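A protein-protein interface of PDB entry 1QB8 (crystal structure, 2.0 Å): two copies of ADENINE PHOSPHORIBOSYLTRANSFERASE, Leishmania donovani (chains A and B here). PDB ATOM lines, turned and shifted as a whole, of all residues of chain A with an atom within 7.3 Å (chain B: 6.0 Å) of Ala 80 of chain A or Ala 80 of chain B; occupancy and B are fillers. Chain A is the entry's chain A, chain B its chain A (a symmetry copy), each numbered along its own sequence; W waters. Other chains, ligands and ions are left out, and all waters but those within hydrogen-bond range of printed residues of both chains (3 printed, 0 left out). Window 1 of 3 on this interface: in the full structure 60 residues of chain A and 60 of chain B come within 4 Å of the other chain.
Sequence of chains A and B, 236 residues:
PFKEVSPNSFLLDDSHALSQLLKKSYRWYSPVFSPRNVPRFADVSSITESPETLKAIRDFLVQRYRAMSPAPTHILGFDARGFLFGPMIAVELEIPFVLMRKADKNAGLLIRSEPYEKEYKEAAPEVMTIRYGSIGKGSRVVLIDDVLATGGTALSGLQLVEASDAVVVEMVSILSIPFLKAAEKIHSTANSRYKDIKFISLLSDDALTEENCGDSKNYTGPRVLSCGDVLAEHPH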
ATOM      1  N   GLY A  77     -16.052 -19.377 -10.639  1.00  0.00           N
ATOM      2  CA  GLY A  77     -15.769 -18.986  -9.269  1.00  0.00           C
ATOM      3  C   GLY A  77     -14.337 -18.541  -9.091  1.00  0.00           C
ATOM      4  O   GLY A  77     -13.428 -19.095  -9.704  1.00  0.00           O
ATOM      5  N   PHE A  78     -14.139 -17.567  -8.208  1.00  0.00           N
ATOM      6  CA  PHE A  78     -12.821 -17.004  -7.946  1.00  0.00           C
ATOM      7  C   PHE A  78     -12.074 -17.750  -6.836  1.00  0.00           C
ATOM      8  O   PHE A  78     -12.649 -18.086  -5.802  1.00  0.00           O
ATOM      9  CB  PHE A  78     -12.955 -15.512  -7.581  1.00  0.00           C
ATOM     10  CG  PHE A  78     -13.650 -14.662  -8.637  1.00  0.00           C
ATOM     11  CD1 PHE A  78     -14.003 -15.185  -9.882  1.00  0.00           C
ATOM     12  CD2 PHE A  78     -13.951 -13.325  -8.371  1.00  0.00           C
ATOM     13  CE1 PHE A  78     -14.641 -14.394 -10.840  1.00  0.00           C
ATOM     14  CE2 PHE A  78     -14.585 -12.524  -9.319  1.00  0.00           C
ATOM     15  CZ  PHE A  78     -14.933 -13.060 -10.558  1.00  0.00           C
ATOM     16  N   ASP A  79     -10.788 -18.005  -7.070  1.00  0.00           N
ATOM     17  CA  ASP A  79      -9.907 -18.699  -6.121  1.00  0.00           C
ATOM     18  C   ASP A  79      -9.700 -17.812  -4.876  1.00  0.00           C
ATOM     19  O   ASP A  79      -9.272 -16.670  -5.010  1.00  0.00           O
ATOM     20  CB  ASP A  79      -8.560 -18.946  -6.827  1.00  0.00           C
ATOM     21  CG  ASP A  79      -7.626 -19.879  -6.062  1.00  0.00           C
ATOM     22  OD1 ASP A  79      -7.869 -20.198  -4.888  1.00  0.00           O
ATOM     23  OD2 ASP A  79      -6.616 -20.297  -6.654  1.00  0.00           O
ATOM     24  N   ALA A  80     -10.017 -18.297  -3.674  1.00  0.00           N
ATOM     25  CA  ALA A  80     -10.503 -19.650  -3.414  1.00  0.00           C
ATOM     26  C   ALA A  80     -11.914 -19.648  -2.830  1.00  0.00           C
ATOM     27  O   ALA A  80     -12.600 -20.665  -2.853  1.00  0.00           O
ATOM     28  CB  ALA A  80      -9.567 -20.345  -2.425  1.00  0.00           C
ATOM     29  N   ARG A  81     -12.344 -18.515  -2.293  1.00  0.00           N
ATOM     30  CA  ARG A  81     -13.646 -18.460  -1.655  1.00  0.00           C
ATOM     31  C   ARG A  81     -14.843 -18.612  -2.577  1.00  0.00           C
ATOM     32  O   ARG A  81     -15.921 -19.018  -2.139  1.00  0.00           O
ATOM     33  CB  ARG A  81     -13.718 -17.253  -0.725  1.00  0.00           C
ATOM     34  CG  ARG A  81     -12.601 -17.326   0.319  1.00  0.00           C
ATOM     35  CD  ARG A  81     -12.798 -16.376   1.464  1.00  0.00           C
ATOM     36  NE  ARG A  81     -12.384 -15.012   1.163  1.00  0.00           N
ATOM     37  CZ  ARG A  81     -11.278 -14.472   1.651  1.00  0.00           C
ATOM     38  NH1 ARG A  81     -10.940 -13.227   1.363  1.00  0.00           N
ATOM     39  NH2 ARG A  81     -10.493 -15.205   2.418  1.00  0.00           N
ATOM     40  N   GLY A  82     -14.630 -18.353  -3.862  1.00  0.00           N
ATOM     41  CA  GLY A  82     -15.687 -18.538  -4.842  1.00  0.00           C
ATOM     42  C   GLY A  82     -15.897 -20.035  -5.075  1.00  0.00           C
ATOM     43  O   GLY A  82     -16.968 -20.466  -5.501  1.00  0.00           O
ATOM     44  N   PHE A  83     -14.867 -20.828  -4.780  1.00  0.00           N
ATOM     45  CA  PHE A  83     -14.919 -22.286  -4.931  1.00  0.00           C
ATOM     46  C   PHE A  83     -15.886 -22.907  -3.930  1.00  0.00           C
ATOM     47  O   PHE A  83     -16.383 -24.007  -4.139  1.00  0.00           O
ATOM     48  CB  PHE A  83     -13.539 -22.910  -4.691  1.00  0.00           C
ATOM     49  CG  PHE A  83     -12.511 -22.574  -5.742  1.00  0.00           C
ATOM     50  CD1 PHE A  83     -12.830 -21.763  -6.831  1.00  0.00           C
ATOM     51  CD2 PHE A  83     -11.214 -23.085  -5.641  1.00  0.00           C
ATOM     52  CE1 PHE A  83     -11.875 -21.462  -7.808  1.00  0.00           C
ATOM     53  CE2 PHE A  83     -10.250 -22.793  -6.612  1.00  0.00           C
ATOM     54  CZ  PHE A  83     -10.581 -21.978  -7.700  1.00  0.00           C
ATOM     55  N   LEU A  84     -16.128 -22.198  -2.835  1.00  0.00           N
ATOM     56  CA  LEU A  84     -17.013 -22.671  -1.779  1.00  0.00           C
ATOM     57  C   LEU A  84     -18.503 -22.615  -2.108  1.00  0.00           C
ATOM     58  O   LEU A  84     -19.298 -23.355  -1.518  1.00  0.00           O
ATOM     59  CB  LEU A  84     -16.764 -21.870  -0.494  1.00  0.00           C
ATOM     60  CG  LEU A  84     -15.363 -21.929   0.126  1.00  0.00           C
ATOM     61  CD1 LEU A  84     -15.178 -20.745   1.070  1.00  0.00           C
ATOM     62  CD2 LEU A  84     -15.174 -23.252   0.853  1.00  0.00           C
ATOM     63  N   PHE A  85     -18.882 -21.744  -3.037  1.00  0.00           N
ATOM     64  CA  PHE A  85     -20.287 -21.580  -3.381  1.00  0.00           C
ATOM     65  C   PHE A  85     -20.669 -22.003  -4.787  1.00  0.00           C
ATOM     66  O   PHE A  85     -21.781 -22.475  -5.023  1.00  0.00           O
ATOM     67  CB  PHE A  85     -20.691 -20.120  -3.165  1.00  0.00           C
ATOM     68  CG  PHE A  85     -20.352 -19.600  -1.802  1.00  0.00           C
ATOM     69  CD1 PHE A  85     -21.217 -19.811  -0.729  1.00  0.00           C
ATOM     70  CD2 PHE A  85     -19.153 -18.929  -1.581  1.00  0.00           C
ATOM     71  CE1 PHE A  85     -20.891 -19.364   0.549  1.00  0.00           C
ATOM     72  CE2 PHE A  85     -18.815 -18.475  -0.308  1.00  0.00           C
ATOM     73  CZ  PHE A  85     -19.686 -18.693   0.760  1.00  0.00           C
ATOM     74  N   PHE A  97     -18.410 -25.813 -13.821  1.00  0.00           N
ATOM     75  CA  PHE A  97     -17.900 -24.833 -12.873  1.00  0.00           C
ATOM     76  C   PHE A  97     -16.444 -24.635 -13.276  1.00  0.00           C
ATOM     77  O   PHE A  97     -15.638 -25.559 -13.182  1.00  0.00           O
ATOM     78  CB  PHE A  97     -17.953 -25.312 -11.424  1.00  0.00           C
ATOM     79  CG  PHE A  97     -17.260 -24.374 -10.466  1.00  0.00           C
ATOM     80  CD1 PHE A  97     -17.847 -23.161 -10.116  1.00  0.00           C
ATOM     81  CD2 PHE A  97     -15.993 -24.669  -9.971  1.00  0.00           C
ATOM     82  CE1 PHE A  97     -17.184 -22.256  -9.291  1.00  0.00           C
ATOM     83  CE2 PHE A  97     -15.323 -23.772  -9.150  1.00  0.00           C
ATOM     84  CZ  PHE A  97     -15.922 -22.563  -8.810  1.00  0.00           C
ATOM     85  N   LEU A  99     -12.704 -22.579 -13.012  1.00  0.00           N
ATOM     86  CA  LEU A  99     -11.870 -21.972 -11.970  1.00  0.00           C
ATOM     87  C   LEU A  99     -11.013 -20.788 -12.425  1.00  0.00           C
ATOM     88  O   LEU A  99     -10.270 -20.891 -13.404  1.00  0.00           O
ATOM     89  CB  LEU A  99     -10.934 -23.029 -11.356  1.00  0.00           C
ATOM     90  CG  LEU A  99     -11.433 -24.139 -10.423  1.00  0.00           C
ATOM     91  CD1 LEU A  99     -12.448 -25.037 -11.098  1.00  0.00           C
ATOM     92  CD2 LEU A  99     -10.241 -24.958  -9.964  1.00  0.00           C
ATOM     93  N   MET A 100     -11.118 -19.662 -11.718  1.00  0.00           N
ATOM     94  CA  MET A 100     -10.276 -18.502 -12.028  1.00  0.00           C
ATOM     95  C   MET A 100      -9.190 -18.476 -10.950  1.00  0.00           C
ATOM     96  O   MET A 100      -9.478 -18.302  -9.765  1.00  0.00           O
ATOM     97  CB  MET A 100     -11.060 -17.181 -12.030  1.00  0.00           C
ATOM     98  CG  MET A 100     -10.214 -15.996 -12.525  1.00  0.00           C
ATOM     99  SD  MET A 100     -11.074 -14.414 -12.669  1.00  0.00           S
ATOM    100  CE  MET A 100     -10.918 -13.799 -11.038  1.00  0.00           C
ATOM    101  N   ARG A 101      -7.949 -18.699 -11.368  1.00  0.00           N
ATOM    102  CA  ARG A 101      -6.819 -18.744 -10.448  1.00  0.00           C
ATOM    103  C   ARG A 101      -5.582 -18.115 -11.070  1.00  0.00           C
ATOM    104  O   ARG A 101      -5.559 -17.807 -12.256  1.00  0.00           O
ATOM    105  CB  ARG A 101      -6.471 -20.204 -10.127  1.00  0.00           C
ATOM    106  CG  ARG A 101      -7.647 -21.180 -10.073  1.00  0.00           C
ATOM    107  CD  ARG A 101      -7.201 -22.528  -9.530  1.00  0.00           C
ATOM    108  NE  ARG A 101      -6.714 -22.391  -8.162  1.00  0.00           N
ATOM    109  CZ  ARG A 101      -6.235 -23.383  -7.416  1.00  0.00           C
ATOM    110  NH1 ARG A 101      -5.825 -23.132  -6.175  1.00  0.00           N
ATOM    111  NH2 ARG A 101      -6.147 -24.616  -7.907  1.00  0.00           N
ATOM    112  N   LYS A 105      -1.271 -21.788 -10.559  1.00  0.00           N
ATOM    113  CA  LYS A 105      -2.217 -22.696  -9.914  1.00  0.00           C
ATOM    114  C   LYS A 105      -3.100 -23.434 -10.921  1.00  0.00           C
ATOM    115  O   LYS A 105      -3.669 -24.472 -10.593  1.00  0.00           O
ATOM    116  CB  LYS A 105      -3.106 -21.929  -8.923  1.00  0.00           C
ATOM    117  CG  LYS A 105      -2.397 -21.446  -7.665  1.00  0.00           C
ATOM    118  CD  LYS A 105      -1.997 -22.617  -6.766  1.00  0.00           C
ATOM    119  CE  LYS A 105      -1.146 -22.164  -5.575  1.00  0.00           C
ATOM    120  NZ  LYS A 105      -1.845 -21.148  -4.724  1.00  0.00           N
ATOM    121  N   MET A 128      -5.025 -12.890 -13.011  1.00  0.00           N
ATOM    122  CA  MET A 128      -5.782 -14.136 -12.889  1.00  0.00           C
ATOM    123  C   MET A 128      -5.910 -14.833 -14.238  1.00  0.00           C
ATOM    124  O   MET A 128      -5.703 -14.212 -15.276  1.00  0.00           O
ATOM    125  CB  MET A 128      -7.174 -13.852 -12.314  1.00  0.00           C
ATOM    126  CG  MET A 128      -7.170 -13.277 -10.899  1.00  0.00           C
ATOM    127  SD  MET A 128      -6.404 -14.396  -9.722  1.00  0.00           S
ATOM    128  CE  MET A 128      -7.766 -15.432  -9.313  1.00  0.00           C
ATOM    129  N   ASP A 145     -17.975 -14.980  -6.088  1.00  0.00           N
ATOM    130  CA  ASP A 145     -16.942 -14.866  -5.060  1.00  0.00           C
ATOM    131  C   ASP A 145     -17.680 -14.531  -3.762  1.00  0.00           C
ATOM    132  O   ASP A 145     -18.873 -14.211  -3.800  1.00  0.00           O
ATOM    133  CB  ASP A 145     -15.969 -13.741  -5.408  1.00  0.00           C
ATOM    134  CG  ASP A 145     -14.635 -13.872  -4.689  1.00  0.00           C
ATOM    135  OD1 ASP A 145     -13.746 -13.052  -4.967  1.00  0.00           O
ATOM    136  OD2 ASP A 145     -14.451 -14.802  -3.878  1.00  0.00           O
ATOM    137  N   ASP A 146     -16.996 -14.595  -2.619  1.00  0.00           N
ATOM    138  CA  ASP A 146     -17.665 -14.292  -1.355  1.00  0.00           C
ATOM    139  C   ASP A 146     -17.861 -12.805  -1.066  1.00  0.00           C
ATOM    140  O   ASP A 146     -18.976 -12.376  -0.774  1.00  0.00           O
ATOM    141  CB  ASP A 146     -16.989 -14.996  -0.168  1.00  0.00           C
ATOM    142  CG  ASP A 146     -15.631 -14.414   0.177  1.00  0.00           C
ATOM    143  OD1 ASP A 146     -15.271 -14.442   1.378  1.00  0.00           O
ATOM    144  OD2 ASP A 146     -14.921 -13.947  -0.741  1.00  0.00           O
ATOM    145  N   PHE B  78      -9.450 -29.070   2.350  1.00  0.00           N
ATOM    146  CA  PHE B  78      -8.140 -28.448   2.214  1.00  0.00           C
ATOM    147  C   PHE B  78      -8.119 -27.354   1.140  1.00  0.00           C
ATOM    148  O   PHE B  78      -8.667 -27.525   0.052  1.00  0.00           O
ATOM    149  CB  PHE B  78      -7.083 -29.522   1.893  1.00  0.00           C
ATOM    150  CG  PHE B  78      -6.987 -30.644   2.919  1.00  0.00           C
ATOM    151  CD1 PHE B  78      -7.710 -30.605   4.113  1.00  0.00           C
ATOM    152  CD2 PHE B  78      -6.164 -31.744   2.679  1.00  0.00           C
ATOM    153  CE1 PHE B  78      -7.613 -31.641   5.046  1.00  0.00           C
ATOM    154  CE2 PHE B  78      -6.057 -32.784   3.601  1.00  0.00           C
ATOM    155  CZ  PHE B  78      -6.784 -32.733   4.789  1.00  0.00           C
ATOM    156  N   ASP B  79      -7.481 -26.231   1.465  1.00  0.00           N
ATOM    157  CA  ASP B  79      -7.346 -25.078   0.565  1.00  0.00           C
ATOM    158  C   ASP B  79      -6.447 -25.467  -0.628  1.00  0.00           C
ATOM    159  O   ASP B  79      -5.321 -25.907  -0.420  1.00  0.00           O
ATOM    160  CB  ASP B  79      -6.700 -23.932   1.366  1.00  0.00           C
ATOM    161  CG  ASP B  79      -6.722 -22.589   0.643  1.00  0.00           C
ATOM    162  OD1 ASP B  79      -7.028 -22.517  -0.557  1.00  0.00           O
ATOM    163  OD2 ASP B  79      -6.418 -21.576   1.299  1.00  0.00           O
ATOM    164  N   ALA B  80      -6.924 -25.340  -1.868  1.00  0.00           N
ATOM    165  CA  ALA B  80      -8.236 -24.799  -2.213  1.00  0.00           C
ATOM    166  C   ALA B  80      -9.118 -25.835  -2.906  1.00  0.00           C
ATOM    167  O   ALA B  80     -10.333 -25.676  -2.974  1.00  0.00           O
ATOM    168  CB  ALA B  80      -8.063 -23.602  -3.149  1.00  0.00           C
ATOM    169  N   ARG B  81      -8.511 -26.888  -3.434  1.00  0.00           N
ATOM    170  CA  ARG B  81      -9.277 -27.877  -4.171  1.00  0.00           C
ATOM    171  C   ARG B  81     -10.252 -28.705  -3.353  1.00  0.00           C
ATOM    172  O   ARG B  81     -11.230 -29.227  -3.888  1.00  0.00           O
ATOM    173  CB  ARG B  81      -8.346 -28.696  -5.060  1.00  0.00           C
ATOM    174  CG  ARG B  81      -7.583 -27.775  -6.015  1.00  0.00           C
ATOM    175  CD  ARG B  81      -6.912 -28.511  -7.138  1.00  0.00           C
ATOM    176  NE  ARG B  81      -5.643 -29.115  -6.756  1.00  0.00           N
ATOM    177  CZ  ARG B  81      -4.471 -28.628  -7.136  1.00  0.00           C
ATOM    178  NH1 ARG B  81      -3.340 -29.209  -6.778  1.00  0.00           N
ATOM    179  NH2 ARG B  81      -4.443 -27.528  -7.864  1.00  0.00           N
ATOM    180  N   GLY B  82     -10.018 -28.763  -2.046  1.00  0.00           N
ATOM    181  CA  GLY B  82     -10.931 -29.466  -1.160  1.00  0.00           C
ATOM    182  C   GLY B  82     -12.207 -28.640  -0.998  1.00  0.00           C
ATOM    183  O   GLY B  82     -13.268 -29.171  -0.673  1.00  0.00           O
ATOM    184  N   PHE B  83     -12.099 -27.334  -1.238  1.00  0.00           N
ATOM    185  CA  PHE B  83     -13.237 -26.413  -1.144  1.00  0.00           C
ATOM    186  C   PHE B  83     -14.259 -26.689  -2.239  1.00  0.00           C
ATOM    187  O   PHE B  83     -15.427 -26.340  -2.109  1.00  0.00           O
ATOM    188  CB  PHE B  83     -12.776 -24.957  -1.296  1.00  0.00           C
ATOM    189  CG  PHE B  83     -11.931 -24.448  -0.157  1.00  0.00           C
ATOM    190  CD1 PHE B  83     -11.620 -25.263   0.932  1.00  0.00           C
ATOM    191  CD2 PHE B  83     -11.451 -23.135  -0.173  1.00  0.00           C
ATOM    192  CE1 PHE B  83     -10.842 -24.782   1.992  1.00  0.00           C
ATOM    193  CE2 PHE B  83     -10.675 -22.642   0.880  1.00  0.00           C
ATOM    194  CZ  PHE B  83     -10.369 -23.469   1.968  1.00  0.00           C
ATOM    195  N   LEU B  84     -13.802 -27.300  -3.324  1.00  0.00           N
ATOM    196  CA  LEU B  84     -14.655 -27.612  -4.463  1.00  0.00           C
ATOM    197  C   LEU B  84     -15.621 -28.777  -4.251  1.00  0.00           C
ATOM    198  O   LEU B  84     -16.652 -28.861  -4.928  1.00  0.00           O
ATOM    199  CB  LEU B  84     -13.790 -27.910  -5.695  1.00  0.00           C
ATOM    200  CG  LEU B  84     -12.863 -26.801  -6.204  1.00  0.00           C
ATOM    201  CD1 LEU B  84     -11.781 -27.413  -7.088  1.00  0.00           C
ATOM    202  CD2 LEU B  84     -13.671 -25.757  -6.961  1.00  0.00           C
ATOM    203  N   ARG B 101      -6.471 -23.800   5.946  1.00  0.00           N
ATOM    204  CA  ARG B 101      -5.688 -22.891   5.117  1.00  0.00           C
ATOM    205  C   ARG B 101      -4.451 -22.405   5.857  1.00  0.00           C
ATOM    206  O   ARG B 101      -4.300 -22.633   7.052  1.00  0.00           O
ATOM    207  CB  ARG B 101      -6.525 -21.653   4.773  1.00  0.00           C
ATOM    208  CG  ARG B 101      -8.026 -21.885   4.592  1.00  0.00           C
ATOM    209  CD  ARG B 101      -8.699 -20.640   4.037  1.00  0.00           C
ATOM    210  NE  ARG B 101      -8.168 -20.316   2.718  1.00  0.00           N
ATOM    211  CZ  ARG B 101      -8.535 -19.274   1.978  1.00  0.00           C
ATOM    212  NH1 ARG B 101      -7.980 -19.090   0.783  1.00  0.00           N
ATOM    213  NH2 ARG B 101      -9.439 -18.410   2.430  1.00  0.00           N
ATOM    214  N   ASP B 145      -9.873 -33.579   0.028  1.00  0.00           N
ATOM    215  CA  ASP B 145      -9.027 -32.845  -0.911  1.00  0.00           C
ATOM    216  C   ASP B 145      -9.158 -33.574  -2.251  1.00  0.00           C
ATOM    217  O   ASP B 145      -9.707 -34.679  -2.295  1.00  0.00           O
ATOM    218  CB  ASP B 145      -7.570 -32.874  -0.448  1.00  0.00           C
ATOM    219  CG  ASP B 145      -6.733 -31.763  -1.063  1.00  0.00           C
ATOM    220  OD1 ASP B 145      -5.556 -31.650  -0.687  1.00  0.00           O
ATOM    221  OD2 ASP B 145      -7.244 -30.980  -1.890  1.00  0.00           O
HETATM  222  O   HOH W   1     -10.628 -17.326   4.837  1.00  0.00           O
HETATM  223  O   HOH W   2      -5.928 -26.138 -10.360  1.00  0.00           O
HETATM  224  O   HOH W   3      -2.572 -25.896  -8.351  1.00  0.00           O
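NH2 of Arg 81 of chain A lies close to NH2 of Arg 101 of chain B, at 3.4 Å. The backbone carbonyl oxygen (O) of Phe 83 of chain B lies close to the backbone carbonyl oxygen (O) of Phe 83 of chain A (3.2 Å). The guanidinium group of Arg 81 of chain B lies close to the guanidinium group of Arg 101 of chain A (3.4 Å).
The backbone carbonyl oxygen (O) of Met 100 of chain A is in hydrogen-bond range of the backbone NH (N) of Asp 79 of chain A, at 3.0 Å. The side-chain carboxylate (OD2) of Asp 79 of chain A lies within salt-bridge range of the guanidinium group (NE) of Arg 101 of chain A (2.6 Å). OD1 of Asp 146 of chain A is in salt-bridge range of NE of Arg 81 of chain A. The guanidinium group of Arg 101 of chain B lies within salt-bridge range of the side-chain carboxylate of Asp 79 of chain B (2.6 Å).
Among the printed residues, merely in contact across the chains: Phe 97 of chain A with Leu 84 of chain B (3.4 Å), Phe 83 of chain A with Leu 84 of chain B (3.6 Å), Leu 84 of chain A with Phe 83 of chain B (3.6 Å), Ala 80 of chain A with Ala 80 of chain B (3.7 Å), Ala 80 of chain A with Arg 101 of chain B (3.8 Å), Arg 101 of chain A with Ala 80 of chain B (3.8 Å), Phe 83 of chain A with Ala 80 of chain B (3.8 Å), Ala 80 of chain A with Phe 83 of chain B (3.8 Å), Asp 79 of chain A with Ala 80 of chain B (3.8 Å) and Ala 80 of chain A with Asp 79 of chain B (3.8 Å).
Printed residues of chain B within 4 Å of Asp 79 of chain A: Ala 80. Of chain B, only Asp 79, Ala 80, Phe 83 and Arg 101 come within 4 Å of Ala 80 of chain A. Of the printed residues of chain B, Leu 84 of chain A touches Phe 83. Of the printed residues of chain B, Arg 101 of chain A touches Ala 80 and Arg 81. Ala 80 of chain B touches four residues of chain A. Of the printed residues of chain A, Leu 84 of chain B touches Phe 83 (3.6 Å) and Phe 97 (3.4 Å). The nearest printed residue of chain B that does not touch Ala 80 of chain A is Leu 84 of chain B (6.6 Å). The nearest residue of chain A that does not touch Ala 80 of chain B is Leu 84 of chain A (6.6 Å). The nearest printed residue of chain B that does not touch Arg 81 of chain A is Phe 83 of chain B (5.2 Å).
Of the 9 printed residues of chain B, 6 touch a printed residue of chain A. Hydrophobic or aromatic side chains of chain B within 4 Å of the printed part of chain A: Ala 80, Phe 83 and Leu 84. Among the printed residues, 13 pairs touch across the chains. Among the printed residues, no Asp or Glu carboxylate lies within 4 Å of a Lys or Arg side-chain nitrogen of the other chain.
Asp 79 of chain A touches Ala 80 of chain B, and with the chains exchanged Ala 80 of chain A touches Asp 79 of chain B. Ala 80 of chain B touches its own counterpart, Ala 80 of chain A. Arg 81 of chain A touches Arg 101 of chain B, and with the chains exchanged Arg 101 of chain A touches Arg 81 of chain B. Phe 83 of chain A touches its own counterpart, Phe 83 of chain B. Positions printed for both chains: 78, 79, 80, 81, 82, 83, 84, 101 and 145.
Water W3 bridges NH2 of Arg 81 of chain B (2.5 Å) and O of Lys 105 of chain A (2.9 Å). Water W2 lies within hydrogen-bond range of O of Lys 105 of chain A, NH2 of Arg 101 of chain A and NH2 of Arg 81 of chain B. Water W1 lies within hydrogen-bond range of NH2 of Arg 101 of chain B and NH2 of Arg 81 of chain A.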
